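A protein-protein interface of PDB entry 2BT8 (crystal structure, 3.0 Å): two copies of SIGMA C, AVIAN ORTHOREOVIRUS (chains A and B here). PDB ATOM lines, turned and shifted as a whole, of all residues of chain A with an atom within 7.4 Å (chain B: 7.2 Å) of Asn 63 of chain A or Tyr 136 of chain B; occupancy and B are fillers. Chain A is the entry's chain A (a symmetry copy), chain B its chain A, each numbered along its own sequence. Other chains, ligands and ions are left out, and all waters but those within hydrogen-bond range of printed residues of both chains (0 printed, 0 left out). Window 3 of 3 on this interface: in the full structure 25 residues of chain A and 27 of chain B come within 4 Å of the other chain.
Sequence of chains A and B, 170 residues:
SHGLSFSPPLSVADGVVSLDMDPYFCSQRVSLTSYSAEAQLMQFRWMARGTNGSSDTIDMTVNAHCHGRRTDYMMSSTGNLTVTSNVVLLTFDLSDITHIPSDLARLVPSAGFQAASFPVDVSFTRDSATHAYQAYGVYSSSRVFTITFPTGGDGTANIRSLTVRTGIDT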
ATOM      1  N   LEU A  41     -13.227 -27.235  28.356  1.00  0.00           N
ATOM      2  CA  LEU A  41     -12.531 -26.645  27.231  1.00  0.00           C
ATOM      3  C   LEU A  41     -13.537 -25.884  26.373  1.00  0.00           C
ATOM      4  O   LEU A  41     -14.247 -26.492  25.623  1.00  0.00           O
ATOM      5  CB  LEU A  41     -11.826 -27.739  26.428  1.00  0.00           C
ATOM      6  CG  LEU A  41     -10.955 -27.240  25.276  1.00  0.00           C
ATOM      7  CD1 LEU A  41      -9.713 -26.588  25.842  1.00  0.00           C
ATOM      8  CD2 LEU A  41     -10.588 -28.349  24.290  1.00  0.00           C
ATOM      9  N   MET A  42     -13.618 -24.564  26.506  1.00  0.00           N
ATOM     10  CA  MET A  42     -14.515 -23.749  25.660  1.00  0.00           C
ATOM     11  C   MET A  42     -13.887 -23.421  24.288  1.00  0.00           C
ATOM     12  O   MET A  42     -12.680 -23.164  24.205  1.00  0.00           O
ATOM     13  CB  MET A  42     -14.878 -22.429  26.353  1.00  0.00           C
ATOM     14  CG  MET A  42     -15.537 -22.527  27.723  1.00  0.00           C
ATOM     15  SD  MET A  42     -15.068 -21.031  28.634  1.00  0.00           S
ATOM     16  CE  MET A  42     -15.650 -21.361  30.299  1.00  0.00           C
ATOM     17  N   GLN A  43     -14.693 -23.419  23.225  1.00  0.00           N
ATOM     18  CA  GLN A  43     -14.217 -23.007  21.907  1.00  0.00           C
ATOM     19  C   GLN A  43     -15.138 -21.935  21.360  1.00  0.00           C
ATOM     20  O   GLN A  43     -16.311 -22.156  21.263  1.00  0.00           O
ATOM     21  CB  GLN A  43     -14.175 -24.186  20.949  1.00  0.00           C
ATOM     22  CG  GLN A  43     -14.054 -25.561  21.651  1.00  0.00           C
ATOM     23  CD  GLN A  43     -13.630 -26.718  20.696  1.00  0.00           C
ATOM     24  OE1 GLN A  43     -13.477 -27.877  21.122  1.00  0.00           O
ATOM     25  NE2 GLN A  43     -13.423 -26.390  19.405  1.00  0.00           N
ATOM     26  N   PHE A  44     -14.613 -20.778  20.998  1.00  0.00           N
ATOM     27  CA  PHE A  44     -15.437 -19.666  20.529  1.00  0.00           C
ATOM     28  C   PHE A  44     -14.604 -18.703  19.694  1.00  0.00           C
ATOM     29  O   PHE A  44     -13.382 -18.881  19.548  1.00  0.00           O
ATOM     30  CB  PHE A  44     -16.051 -18.918  21.714  1.00  0.00           C
ATOM     31  CG  PHE A  44     -15.043 -18.481  22.742  1.00  0.00           C
ATOM     32  CD1 PHE A  44     -14.420 -17.237  22.647  1.00  0.00           C
ATOM     33  CD2 PHE A  44     -14.695 -19.325  23.802  1.00  0.00           C
ATOM     34  CE1 PHE A  44     -13.446 -16.829  23.595  1.00  0.00           C
ATOM     35  CE2 PHE A  44     -13.746 -18.919  24.763  1.00  0.00           C
ATOM     36  CZ  PHE A  44     -13.119 -17.660  24.641  1.00  0.00           C
ATOM     37  N   MET A  60     -10.201 -14.306  16.046  1.00  0.00           N
ATOM     38  CA  MET A  60      -9.348 -15.350  16.584  1.00  0.00           C
ATOM     39  C   MET A  60     -10.246 -16.506  16.959  1.00  0.00           C
ATOM     40  O   MET A  60     -11.319 -16.315  17.550  1.00  0.00           O
ATOM     41  CB  MET A  60      -8.610 -14.877  17.818  1.00  0.00           C
ATOM     42  CG  MET A  60      -7.881 -13.557  17.669  1.00  0.00           C
ATOM     43  SD  MET A  60      -6.328 -13.631  16.719  1.00  0.00           S
ATOM     44  CE  MET A  60      -5.419 -14.989  17.464  1.00  0.00           C
ATOM     45  N   THR A  61      -9.832 -17.704  16.581  1.00  0.00           N
ATOM     46  CA  THR A  61     -10.497 -18.901  17.042  1.00  0.00           C
ATOM     47  C   THR A  61      -9.861 -19.216  18.358  1.00  0.00           C
ATOM     48  O   THR A  61      -8.654 -19.461  18.405  1.00  0.00           O
ATOM     49  CB  THR A  61     -10.194 -20.067  16.125  1.00  0.00           C
ATOM     50  OG1 THR A  61     -10.525 -19.697  14.783  1.00  0.00           O
ATOM     51  CG2 THR A  61     -10.956 -21.347  16.566  1.00  0.00           C
ATOM     52  N   VAL A  62     -10.651 -19.246  19.424  1.00  0.00           N
ATOM     53  CA  VAL A  62     -10.062 -19.456  20.747  1.00  0.00           C
ATOM     54  C   VAL A  62     -10.400 -20.788  21.389  1.00  0.00           C
ATOM     55  O   VAL A  62     -11.538 -21.217  21.343  1.00  0.00           O
ATOM     56  CB  VAL A  62     -10.462 -18.353  21.707  1.00  0.00           C
ATOM     57  CG1 VAL A  62      -9.965 -18.693  23.097  1.00  0.00           C
ATOM     58  CG2 VAL A  62      -9.898 -17.023  21.229  1.00  0.00           C
ATOM     59  N   ASN A  63      -9.415 -21.443  21.987  1.00  0.00           N
ATOM     60  CA  ASN A  63      -9.748 -22.503  22.906  1.00  0.00           C
ATOM     61  C   ASN A  63      -9.307 -22.097  24.264  1.00  0.00           C
ATOM     62  O   ASN A  63      -8.130 -21.777  24.443  1.00  0.00           O
ATOM     63  CB  ASN A  63      -9.081 -23.816  22.551  1.00  0.00           C
ATOM     64  CG  ASN A  63      -9.712 -24.469  21.357  1.00  0.00           C
ATOM     65  OD1 ASN A  63      -9.577 -23.969  20.254  1.00  0.00           O
ATOM     66  ND2 ASN A  63     -10.397 -25.594  21.562  1.00  0.00           N
ATOM     67  N   ALA A  64     -10.243 -22.089  25.213  1.00  0.00           N
ATOM     68  CA  ALA A  64      -9.903 -21.818  26.608  1.00  0.00           C
ATOM     69  C   ALA A  64     -10.060 -23.074  27.463  1.00  0.00           C
ATOM     70  O   ALA A  64     -11.123 -23.682  27.503  1.00  0.00           O
ATOM     71  CB  ALA A  64     -10.725 -20.670  27.155  1.00  0.00           C
ATOM     72  N   HIS A  65      -8.981 -23.482  28.113  1.00  0.00           N
ATOM     73  CA  HIS A  65      -9.009 -24.645  28.976  1.00  0.00           C
ATOM     74  C   HIS A  65      -9.064 -24.059  30.372  1.00  0.00           C
ATOM     75  O   HIS A  65      -8.048 -23.546  30.889  1.00  0.00           O
ATOM     76  CB  HIS A  65      -7.753 -25.461  28.736  1.00  0.00           C
ATOM     77  CG  HIS A  65      -7.654 -26.707  29.555  1.00  0.00           C
ATOM     78  ND1 HIS A  65      -6.514 -27.041  30.264  1.00  0.00           N
ATOM     79  CD2 HIS A  65      -8.526 -27.720  29.749  1.00  0.00           C
ATOM     80  CE1 HIS A  65      -6.701 -28.200  30.871  1.00  0.00           C
ATOM     81  NE2 HIS A  65      -7.912 -28.636  30.570  1.00  0.00           N
ATOM     82  N   CYS A  66     -10.287 -24.052  30.926  1.00  0.00           N
ATOM     83  CA  CYS A  66     -10.584 -23.598  32.289  1.00  0.00           C
ATOM     84  C   CYS A  66     -10.478 -24.836  33.189  1.00  0.00           C
ATOM     85  O   CYS A  66     -11.340 -25.715  33.139  1.00  0.00           O
ATOM     86  CB  CYS A  66     -11.993 -23.023  32.356  1.00  0.00           C
ATOM     87  SG  CYS A  66     -12.562 -21.988  30.926  1.00  0.00           S
ATOM     88  N   THR A  71      -6.798 -20.707  33.874  1.00  0.00           N
ATOM     89  CA  THR A  71      -7.417 -20.737  32.530  1.00  0.00           C
ATOM     90  C   THR A  71      -6.431 -20.427  31.433  1.00  0.00           C
ATOM     91  O   THR A  71      -5.864 -19.333  31.418  1.00  0.00           O
ATOM     92  CB  THR A  71      -8.615 -19.820  32.430  1.00  0.00           C
ATOM     93  OG1 THR A  71      -9.627 -20.313  33.318  1.00  0.00           O
ATOM     94  CG2 THR A  71      -9.151 -19.816  31.015  1.00  0.00           C
ATOM     95  N   ASP A  72      -6.217 -21.388  30.531  1.00  0.00           N
ATOM     96  CA  ASP A  72      -5.178 -21.248  29.498  1.00  0.00           C
ATOM     97  C   ASP A  72      -5.774 -20.991  28.121  1.00  0.00           C
ATOM     98  O   ASP A  72      -6.646 -21.735  27.663  1.00  0.00           O
ATOM     99  CB  ASP A  72      -4.271 -22.474  29.467  1.00  0.00           C
ATOM    100  CG  ASP A  72      -3.448 -22.629  30.746  1.00  0.00           C
ATOM    101  OD1 ASP A  72      -2.675 -21.703  31.072  1.00  0.00           O
ATOM    102  OD2 ASP A  72      -3.552 -23.677  31.421  1.00  0.00           O
ATOM    103  N   TYR A  73      -5.320 -19.926  27.468  1.00  0.00           N
ATOM    104  CA  TYR A  73      -5.815 -19.588  26.135  1.00  0.00           C
ATOM    105  C   TYR A  73      -4.884 -20.081  25.012  1.00  0.00           C
ATOM    106  O   TYR A  73      -3.678 -19.815  25.043  1.00  0.00           O
ATOM    107  CB  TYR A  73      -5.938 -18.079  25.983  1.00  0.00           C
ATOM    108  CG  TYR A  73      -7.010 -17.362  26.776  1.00  0.00           C
ATOM    109  CD1 TYR A  73      -8.336 -17.748  26.726  1.00  0.00           C
ATOM    110  CD2 TYR A  73      -6.687 -16.220  27.524  1.00  0.00           C
ATOM    111  CE1 TYR A  73      -9.320 -17.030  27.442  1.00  0.00           C
ATOM    112  CE2 TYR A  73      -7.641 -15.511  28.232  1.00  0.00           C
ATOM    113  CZ  TYR A  73      -8.959 -15.916  28.192  1.00  0.00           C
ATOM    114  OH  TYR A  73      -9.902 -15.195  28.903  1.00  0.00           O
ATOM    115  N   MET A  74      -5.452 -20.769  24.023  1.00  0.00           N
ATOM    116  CA  MET A  74      -4.769 -21.084  22.778  1.00  0.00           C
ATOM    117  C   MET A  74      -5.609 -20.534  21.638  1.00  0.00           C
ATOM    118  O   MET A  74      -6.720 -21.019  21.407  1.00  0.00           O
ATOM    119  CB  MET A  74      -4.702 -22.585  22.585  1.00  0.00           C
ATOM    120  CG  MET A  74      -3.826 -23.370  23.584  1.00  0.00           C
ATOM    121  SD  MET A  74      -4.555 -23.834  25.187  1.00  0.00           S
ATOM    122  CE  MET A  74      -6.203 -24.370  24.766  1.00  0.00           C
ATOM    123  N   MET A  75      -5.074 -19.543  20.921  1.00  0.00           N
ATOM    124  CA  MET A  75      -5.802 -18.837  19.868  1.00  0.00           C
ATOM    125  C   MET A  75      -5.127 -18.761  18.503  1.00  0.00           C
ATOM    126  O   MET A  75      -3.907 -18.714  18.389  1.00  0.00           O
ATOM    127  CB  MET A  75      -6.046 -17.396  20.275  1.00  0.00           C
ATOM    128  CG  MET A  75      -6.051 -17.107  21.756  1.00  0.00           C
ATOM    129  SD  MET A  75      -6.570 -15.389  21.943  1.00  0.00           S
ATOM    130  CE  MET A  75      -7.099 -15.410  23.662  1.00  0.00           C
ATOM    131  N   SER A  76      -5.969 -18.653  17.475  1.00  0.00           N
ATOM    132  CA  SER A  76      -5.582 -18.535  16.073  1.00  0.00           C
ATOM    133  C   SER A  76      -6.395 -17.536  15.305  1.00  0.00           C
ATOM    134  O   SER A  76      -7.629 -17.540  15.357  1.00  0.00           O
ATOM    135  CB  SER A  76      -5.828 -19.833  15.400  1.00  0.00           C
ATOM    136  OG  SER A  76      -4.595 -20.448  15.354  1.00  0.00           O
ATOM    137  N   VAL A 164      -1.734 -16.854  19.585  1.00  0.00           N
ATOM    138  CA  VAL A 164      -1.542 -16.323  20.903  1.00  0.00           C
ATOM    139  C   VAL A 164      -1.693 -17.465  21.897  1.00  0.00           C
ATOM    140  O   VAL A 164      -2.751 -18.108  21.947  1.00  0.00           O
ATOM    141  CB  VAL A 164      -2.569 -15.227  21.209  1.00  0.00           C
ATOM    142  CG1 VAL A 164      -2.419 -14.778  22.643  1.00  0.00           C
ATOM    143  CG2 VAL A 164      -2.384 -14.047  20.260  1.00  0.00           C
ATOM    144  N   THR A 166      -1.393 -18.015  25.956  1.00  0.00           N
ATOM    145  CA  THR A 166      -1.219 -17.438  27.290  1.00  0.00           C
ATOM    146  C   THR A 166      -2.086 -18.116  28.326  1.00  0.00           C
ATOM    147  O   THR A 166      -2.792 -19.077  28.033  1.00  0.00           O
ATOM    148  CB  THR A 166      -1.410 -15.879  27.298  1.00  0.00           C
ATOM    149  OG1 THR A 166      -0.986 -15.360  28.552  1.00  0.00           O
ATOM    150  CG2 THR A 166      -2.849 -15.449  27.057  1.00  0.00           C
ATOM    151  N   SER B 117     -11.533 -32.288  27.583  1.00  0.00           N
ATOM    152  CA  SER B 117     -10.359 -32.468  26.728  1.00  0.00           C
ATOM    153  C   SER B 117      -9.311 -31.446  27.126  1.00  0.00           C
ATOM    154  O   SER B 117      -9.665 -30.351  27.567  1.00  0.00           O
ATOM    155  CB  SER B 117     -10.752 -32.302  25.278  1.00  0.00           C
ATOM    156  OG  SER B 117     -11.569 -33.401  24.946  1.00  0.00           O
ATOM    157  N   PHE B 118      -8.037 -31.797  26.985  1.00  0.00           N
ATOM    158  CA  PHE B 118      -6.955 -30.911  27.426  1.00  0.00           C
ATOM    159  C   PHE B 118      -5.932 -30.690  26.326  1.00  0.00           C
ATOM    160  O   PHE B 118      -5.717 -31.565  25.479  1.00  0.00           O
ATOM    161  CB  PHE B 118      -6.273 -31.484  28.676  1.00  0.00           C
ATOM    162  CG  PHE B 118      -5.875 -32.928  28.539  1.00  0.00           C
ATOM    163  CD1 PHE B 118      -6.795 -33.938  28.782  1.00  0.00           C
ATOM    164  CD2 PHE B 118      -4.583 -33.274  28.121  1.00  0.00           C
ATOM    165  CE1 PHE B 118      -6.437 -35.274  28.638  1.00  0.00           C
ATOM    166  CE2 PHE B 118      -4.197 -34.612  27.978  1.00  0.00           C
ATOM    167  CZ  PHE B 118      -5.123 -35.616  28.235  1.00  0.00           C
ATOM    168  N   PRO B 119      -5.286 -29.513  26.330  1.00  0.00           N
ATOM    169  CA  PRO B 119      -4.253 -29.205  25.335  1.00  0.00           C
ATOM    170  C   PRO B 119      -3.008 -30.122  25.387  1.00  0.00           C
ATOM    171  O   PRO B 119      -2.516 -30.465  26.469  1.00  0.00           O
ATOM    172  CB  PRO B 119      -3.895 -27.736  25.631  1.00  0.00           C
ATOM    173  CG  PRO B 119      -4.288 -27.502  26.973  1.00  0.00           C
ATOM    174  CD  PRO B 119      -5.489 -28.390  27.256  1.00  0.00           C
ATOM    175  N   VAL B 120      -2.542 -30.524  24.202  1.00  0.00           N
ATOM    176  CA  VAL B 120      -1.339 -31.345  24.037  1.00  0.00           C
ATOM    177  C   VAL B 120      -0.467 -30.768  22.918  1.00  0.00           C
ATOM    178  O   VAL B 120      -0.980 -30.514  21.829  1.00  0.00           O
ATOM    179  CB  VAL B 120      -1.718 -32.775  23.672  1.00  0.00           C
ATOM    180  CG1 VAL B 120      -0.486 -33.607  23.442  1.00  0.00           C
ATOM    181  CG2 VAL B 120      -2.512 -33.369  24.780  1.00  0.00           C
ATOM    182  N   ASP B 121       0.827 -30.543  23.179  1.00  0.00           N
ATOM    183  CA  ASP B 121       1.756 -30.109  22.122  1.00  0.00           C
ATOM    184  C   ASP B 121       2.403 -31.278  21.439  1.00  0.00           C
ATOM    185  O   ASP B 121       2.999 -32.158  22.080  1.00  0.00           O
ATOM    186  CB  ASP B 121       2.853 -29.265  22.680  1.00  0.00           C
ATOM    187  CG  ASP B 121       2.428 -27.868  22.916  1.00  0.00           C
ATOM    188  OD1 ASP B 121       1.277 -27.513  22.573  1.00  0.00           O
ATOM    189  OD2 ASP B 121       3.264 -27.113  23.452  1.00  0.00           O
ATOM    190  N   VAL B 122       2.305 -31.294  20.125  1.00  0.00           N
ATOM    191  CA  VAL B 122       2.781 -32.430  19.373  1.00  0.00           C
ATOM    192  C   VAL B 122       3.616 -31.947  18.209  1.00  0.00           C
ATOM    193  O   VAL B 122       3.233 -30.990  17.523  1.00  0.00           O
ATOM    194  CB  VAL B 122       1.598 -33.227  18.850  1.00  0.00           C
ATOM    195  CG1 VAL B 122       1.953 -33.958  17.603  1.00  0.00           C
ATOM    196  CG2 VAL B 122       1.163 -34.181  19.876  1.00  0.00           C
ATOM    197  N   TYR B 133       1.743 -29.406  15.800  1.00  0.00           N
ATOM    198  CA  TYR B 133       0.324 -29.092  15.896  1.00  0.00           C
ATOM    199  C   TYR B 133      -0.085 -28.842  17.316  1.00  0.00           C
ATOM    200  O   TYR B 133       0.473 -29.423  18.253  1.00  0.00           O
ATOM    201  CB  TYR B 133      -0.514 -30.229  15.323  1.00  0.00           C
ATOM    202  CG  TYR B 133      -0.239 -30.491  13.864  1.00  0.00           C
ATOM    203  CD1 TYR B 133      -0.659 -29.598  12.899  1.00  0.00           C
ATOM    204  CD2 TYR B 133       0.449 -31.635  13.454  1.00  0.00           C
ATOM    205  CE1 TYR B 133      -0.410 -29.825  11.562  1.00  0.00           C
ATOM    206  CE2 TYR B 133       0.693 -31.886  12.106  1.00  0.00           C
ATOM    207  CZ  TYR B 133       0.262 -30.966  11.165  1.00  0.00           C
ATOM    208  OH  TYR B 133       0.496 -31.155   9.821  1.00  0.00           O
ATOM    209  N   GLN B 134      -1.044 -27.946  17.474  1.00  0.00           N
ATOM    210  CA  GLN B 134      -1.762 -27.843  18.719  1.00  0.00           C
ATOM    211  C   GLN B 134      -2.755 -29.021  18.725  1.00  0.00           C
ATOM    212  O   GLN B 134      -3.682 -29.028  17.956  1.00  0.00           O
ATOM    213  CB  GLN B 134      -2.491 -26.500  18.771  1.00  0.00           C
ATOM    214  CG  GLN B 134      -3.342 -26.315  20.005  1.00  0.00           C
ATOM    215  CD  GLN B 134      -2.491 -26.265  21.236  1.00  0.00           C
ATOM    216  OE1 GLN B 134      -1.834 -25.257  21.489  1.00  0.00           O
ATOM    217  NE2 GLN B 134      -2.456 -27.362  21.991  1.00  0.00           N
ATOM    218  N   ALA B 135      -2.550 -30.036  19.548  1.00  0.00           N
ATOM    219  CA  ALA B 135      -3.493 -31.149  19.592  1.00  0.00           C
ATOM    220  C   ALA B 135      -4.254 -31.196  20.942  1.00  0.00           C
ATOM    221  O   ALA B 135      -4.082 -30.304  21.788  1.00  0.00           O
ATOM    222  CB  ALA B 135      -2.775 -32.428  19.324  1.00  0.00           C
ATOM    223  N   TYR B 136      -5.105 -32.208  21.142  1.00  0.00           N
ATOM    224  CA  TYR B 136      -5.918 -32.290  22.348  1.00  0.00           C
ATOM    225  C   TYR B 136      -5.990 -33.707  22.820  1.00  0.00           C
ATOM    226  O   TYR B 136      -5.989 -34.638  22.014  1.00  0.00           O
ATOM    227  CB  TYR B 136      -7.318 -31.711  22.110  1.00  0.00           C
ATOM    228  CG  TYR B 136      -7.248 -30.206  21.950  1.00  0.00           C
ATOM    229  CD1 TYR B 136      -7.164 -29.355  23.072  1.00  0.00           C
ATOM    230  CD2 TYR B 136      -7.161 -29.632  20.694  1.00  0.00           C
ATOM    231  CE1 TYR B 136      -7.041 -27.966  22.922  1.00  0.00           C
ATOM    232  CE2 TYR B 136      -7.026 -28.260  20.537  1.00  0.00           C
ATOM    233  CZ  TYR B 136      -6.975 -27.431  21.644  1.00  0.00           C
ATOM    234  OH  TYR B 136      -6.854 -26.076  21.444  1.00  0.00           O
ATOM    235  N   GLY B 137      -5.986 -33.873  24.140  1.00  0.00           N
ATOM    236  CA  GLY B 137      -6.085 -35.188  24.765  1.00  0.00           C
ATOM    237  C   GLY B 137      -7.418 -35.299  25.490  1.00  0.00           C
ATOM    238  O   GLY B 137      -8.040 -34.273  25.864  1.00  0.00           O
ATOM    239  N   VAL B 138      -7.870 -36.540  25.671  1.00  0.00           N
ATOM    240  CA  VAL B 138      -9.004 -36.811  26.533  1.00  0.00           C
ATOM    241  C   VAL B 138      -8.817 -38.138  27.246  1.00  0.00           C
ATOM    242  O   VAL B 138      -8.446 -39.132  26.623  1.00  0.00           O
ATOM    243  CB  VAL B 138     -10.381 -36.696  25.784  1.00  0.00           C
ATOM    244  CG1 VAL B 138     -10.597 -37.841  24.845  1.00  0.00           C
ATOM    245  CG2 VAL B 138     -11.502 -36.622  26.776  1.00  0.00           C
ATOM    246  N   PHE B 145      -5.658 -42.132  28.581  1.00  0.00           N
ATOM    247  CA  PHE B 145      -6.021 -41.003  27.717  1.00  0.00           C
ATOM    248  C   PHE B 145      -5.605 -41.173  26.248  1.00  0.00           C
ATOM    249  O   PHE B 145      -4.718 -41.994  25.912  1.00  0.00           O
ATOM    250  CB  PHE B 145      -5.526 -39.683  28.296  1.00  0.00           C
ATOM    251  CG  PHE B 145      -4.044 -39.530  28.267  1.00  0.00           C
ATOM    252  CD1 PHE B 145      -3.260 -40.038  29.295  1.00  0.00           C
ATOM    253  CD2 PHE B 145      -3.423 -38.868  27.204  1.00  0.00           C
ATOM    254  CE1 PHE B 145      -1.890 -39.879  29.270  1.00  0.00           C
ATOM    255  CE2 PHE B 145      -2.060 -38.723  27.166  1.00  0.00           C
ATOM    256  CZ  PHE B 145      -1.292 -39.214  28.205  1.00  0.00           C
ATOM    257  N   THR B 146      -6.254 -40.396  25.385  1.00  0.00           N
ATOM    258  CA  THR B 146      -5.999 -40.487  23.960  1.00  0.00           C
ATOM    259  C   THR B 146      -5.791 -39.143  23.331  1.00  0.00           C
ATOM    260  O   THR B 146      -6.687 -38.285  23.377  1.00  0.00           O
ATOM    261  CB  THR B 146      -7.139 -41.173  23.254  1.00  0.00           C
ATOM    262  OG1 THR B 146      -7.296 -42.458  23.842  1.00  0.00           O
ATOM    263  CG2 THR B 146      -6.827 -41.350  21.772  1.00  0.00           C
ATOM    264  N   ILE B 147      -4.624 -38.953  22.724  1.00  0.00           N
ATOM    265  CA  ILE B 147      -4.425 -37.721  21.983  1.00  0.00           C
ATOM    266  C   ILE B 147      -4.791 -37.935  20.516  1.00  0.00           C
ATOM    267  O   ILE B 147      -4.723 -39.053  20.001  1.00  0.00           O
ATOM    268  CB  ILE B 147      -3.029 -37.111  22.178  1.00  0.00           C
ATOM    269  CG1 ILE B 147      -1.950 -37.913  21.447  1.00  0.00           C
ATOM    270  CG2 ILE B 147      -2.703 -37.053  23.661  1.00  0.00           C
ATOM    271  CD1 ILE B 147      -0.534 -37.545  21.893  1.00  0.00           C
ATOM    272  N   THR B 148      -5.216 -36.858  19.877  1.00  0.00           N
ATOM    273  CA  THR B 148      -5.641 -36.880  18.502  1.00  0.00           C
ATOM    274  C   THR B 148      -4.870 -35.786  17.830  1.00  0.00           C
ATOM    275  O   THR B 148      -4.884 -34.649  18.305  1.00  0.00           O
ATOM    276  CB  THR B 148      -7.088 -36.484  18.418  1.00  0.00           C
ATOM    277  OG1 THR B 148      -7.849 -37.330  19.286  1.00  0.00           O
ATOM    278  CG2 THR B 148      -7.589 -36.600  17.010  1.00  0.00           C
ATOM    279  N   PHE B 149      -4.183 -36.101  16.744  1.00  0.00           N
ATOM    280  CA  PHE B 149      -3.496 -35.063  16.004  1.00  0.00           C
ATOM    281  C   PHE B 149      -3.418 -35.448  14.550  1.00  0.00           C
ATOM    282  O   PHE B 149      -3.532 -36.651  14.200  1.00  0.00           O
ATOM    283  CB  PHE B 149      -2.108 -34.801  16.570  1.00  0.00           C
ATOM    284  CG  PHE B 149      -1.230 -36.017  16.616  1.00  0.00           C
ATOM    285  CD1 PHE B 149      -1.296 -36.893  17.677  1.00  0.00           C
ATOM    286  CD2 PHE B 149      -0.325 -36.274  15.601  1.00  0.00           C
ATOM    287  CE1 PHE B 149      -0.484 -38.019  17.727  1.00  0.00           C
ATOM    288  CE2 PHE B 149       0.498 -37.401  15.647  1.00  0.00           C
ATOM    289  CZ  PHE B 149       0.414 -38.272  16.715  1.00  0.00           C
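The backbone carbonyl oxygen of Phe 118 of chain B lies within hydrogen-bond range of the backbone NH of Gly 137 of chain B.
NE2 of Gln 134 of chain B lies within hydrogen-bond range of O of Val 120 of chain B.
O of Tyr 136 of chain B sits at hydrogen-bond distance from N of Thr 148 of chain B.
N of Asn 63 of chain A sits at hydrogen-bond distance from O of Met 74 of chain A (2.8 Å).
O of His 65 of chain A sits at hydrogen-bond distance from N of Asp 72 of chain A (2.9 Å).
Among the printed residues, pairs that only touch across the chains: Leu 41 of chain A with Ser 117 of chain B (3.6 Å), Leu 41 of chain A with Tyr 136 of chain B (3.8 Å), Asn 63 of chain A with Tyr 136 of chain B (3.3 Å), His 65 of chain A with Ser 117 of chain B (3.6 Å), His 65 of chain A with Phe 118 of chain B (3.8 Å), His 65 of chain A with Pro 119 of chain B (3.5 Å), Met 74 of chain A with Pro 119 of chain B (3.98 Å), Met 74 of chain A with Gln 134 of chain B (3.5 Å) and Met 74 of chain A with Tyr 136 of chain B (3.8 Å).
Of chain B, only Tyr 136 (3.3 Å) comes within 4 Å of Asn 63 of chain A.
Printed residues of chain B within 4 Å of His 65 of chain A: Ser 117 (3.6 Å), Phe 118 (3.8 Å) and Pro 119 (3.5 Å).
Of the printed residues of chain A, Ser 117 of chain B touches Leu 41 and His 65.
Printed residues of chain A within 4 Å of Pro 119 of chain B: His 65 and Met 74.
Tyr 136 of chain B touches just these residues of chain A: Leu 41, Asn 63 and Met 74.
The nearest printed residue of chain A that does not touch Tyr 136 of chain B is Val 62 of chain A (6.4 Å).
Hydrophobic or aromatic side chains of chain B that line the printed part of chain A: Phe 118, Pro 119 and Tyr 136.
Hydrophobic or aromatic side chains of chain A within 4 Å of the printed part of chain B: Leu 41, His 65 and Met 74.
Among the printed residues, no Asp or Glu carboxylate lies within 4 Å of a Lys or Arg side-chain nitrogen of the other chain.
No position is printed for both chains.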
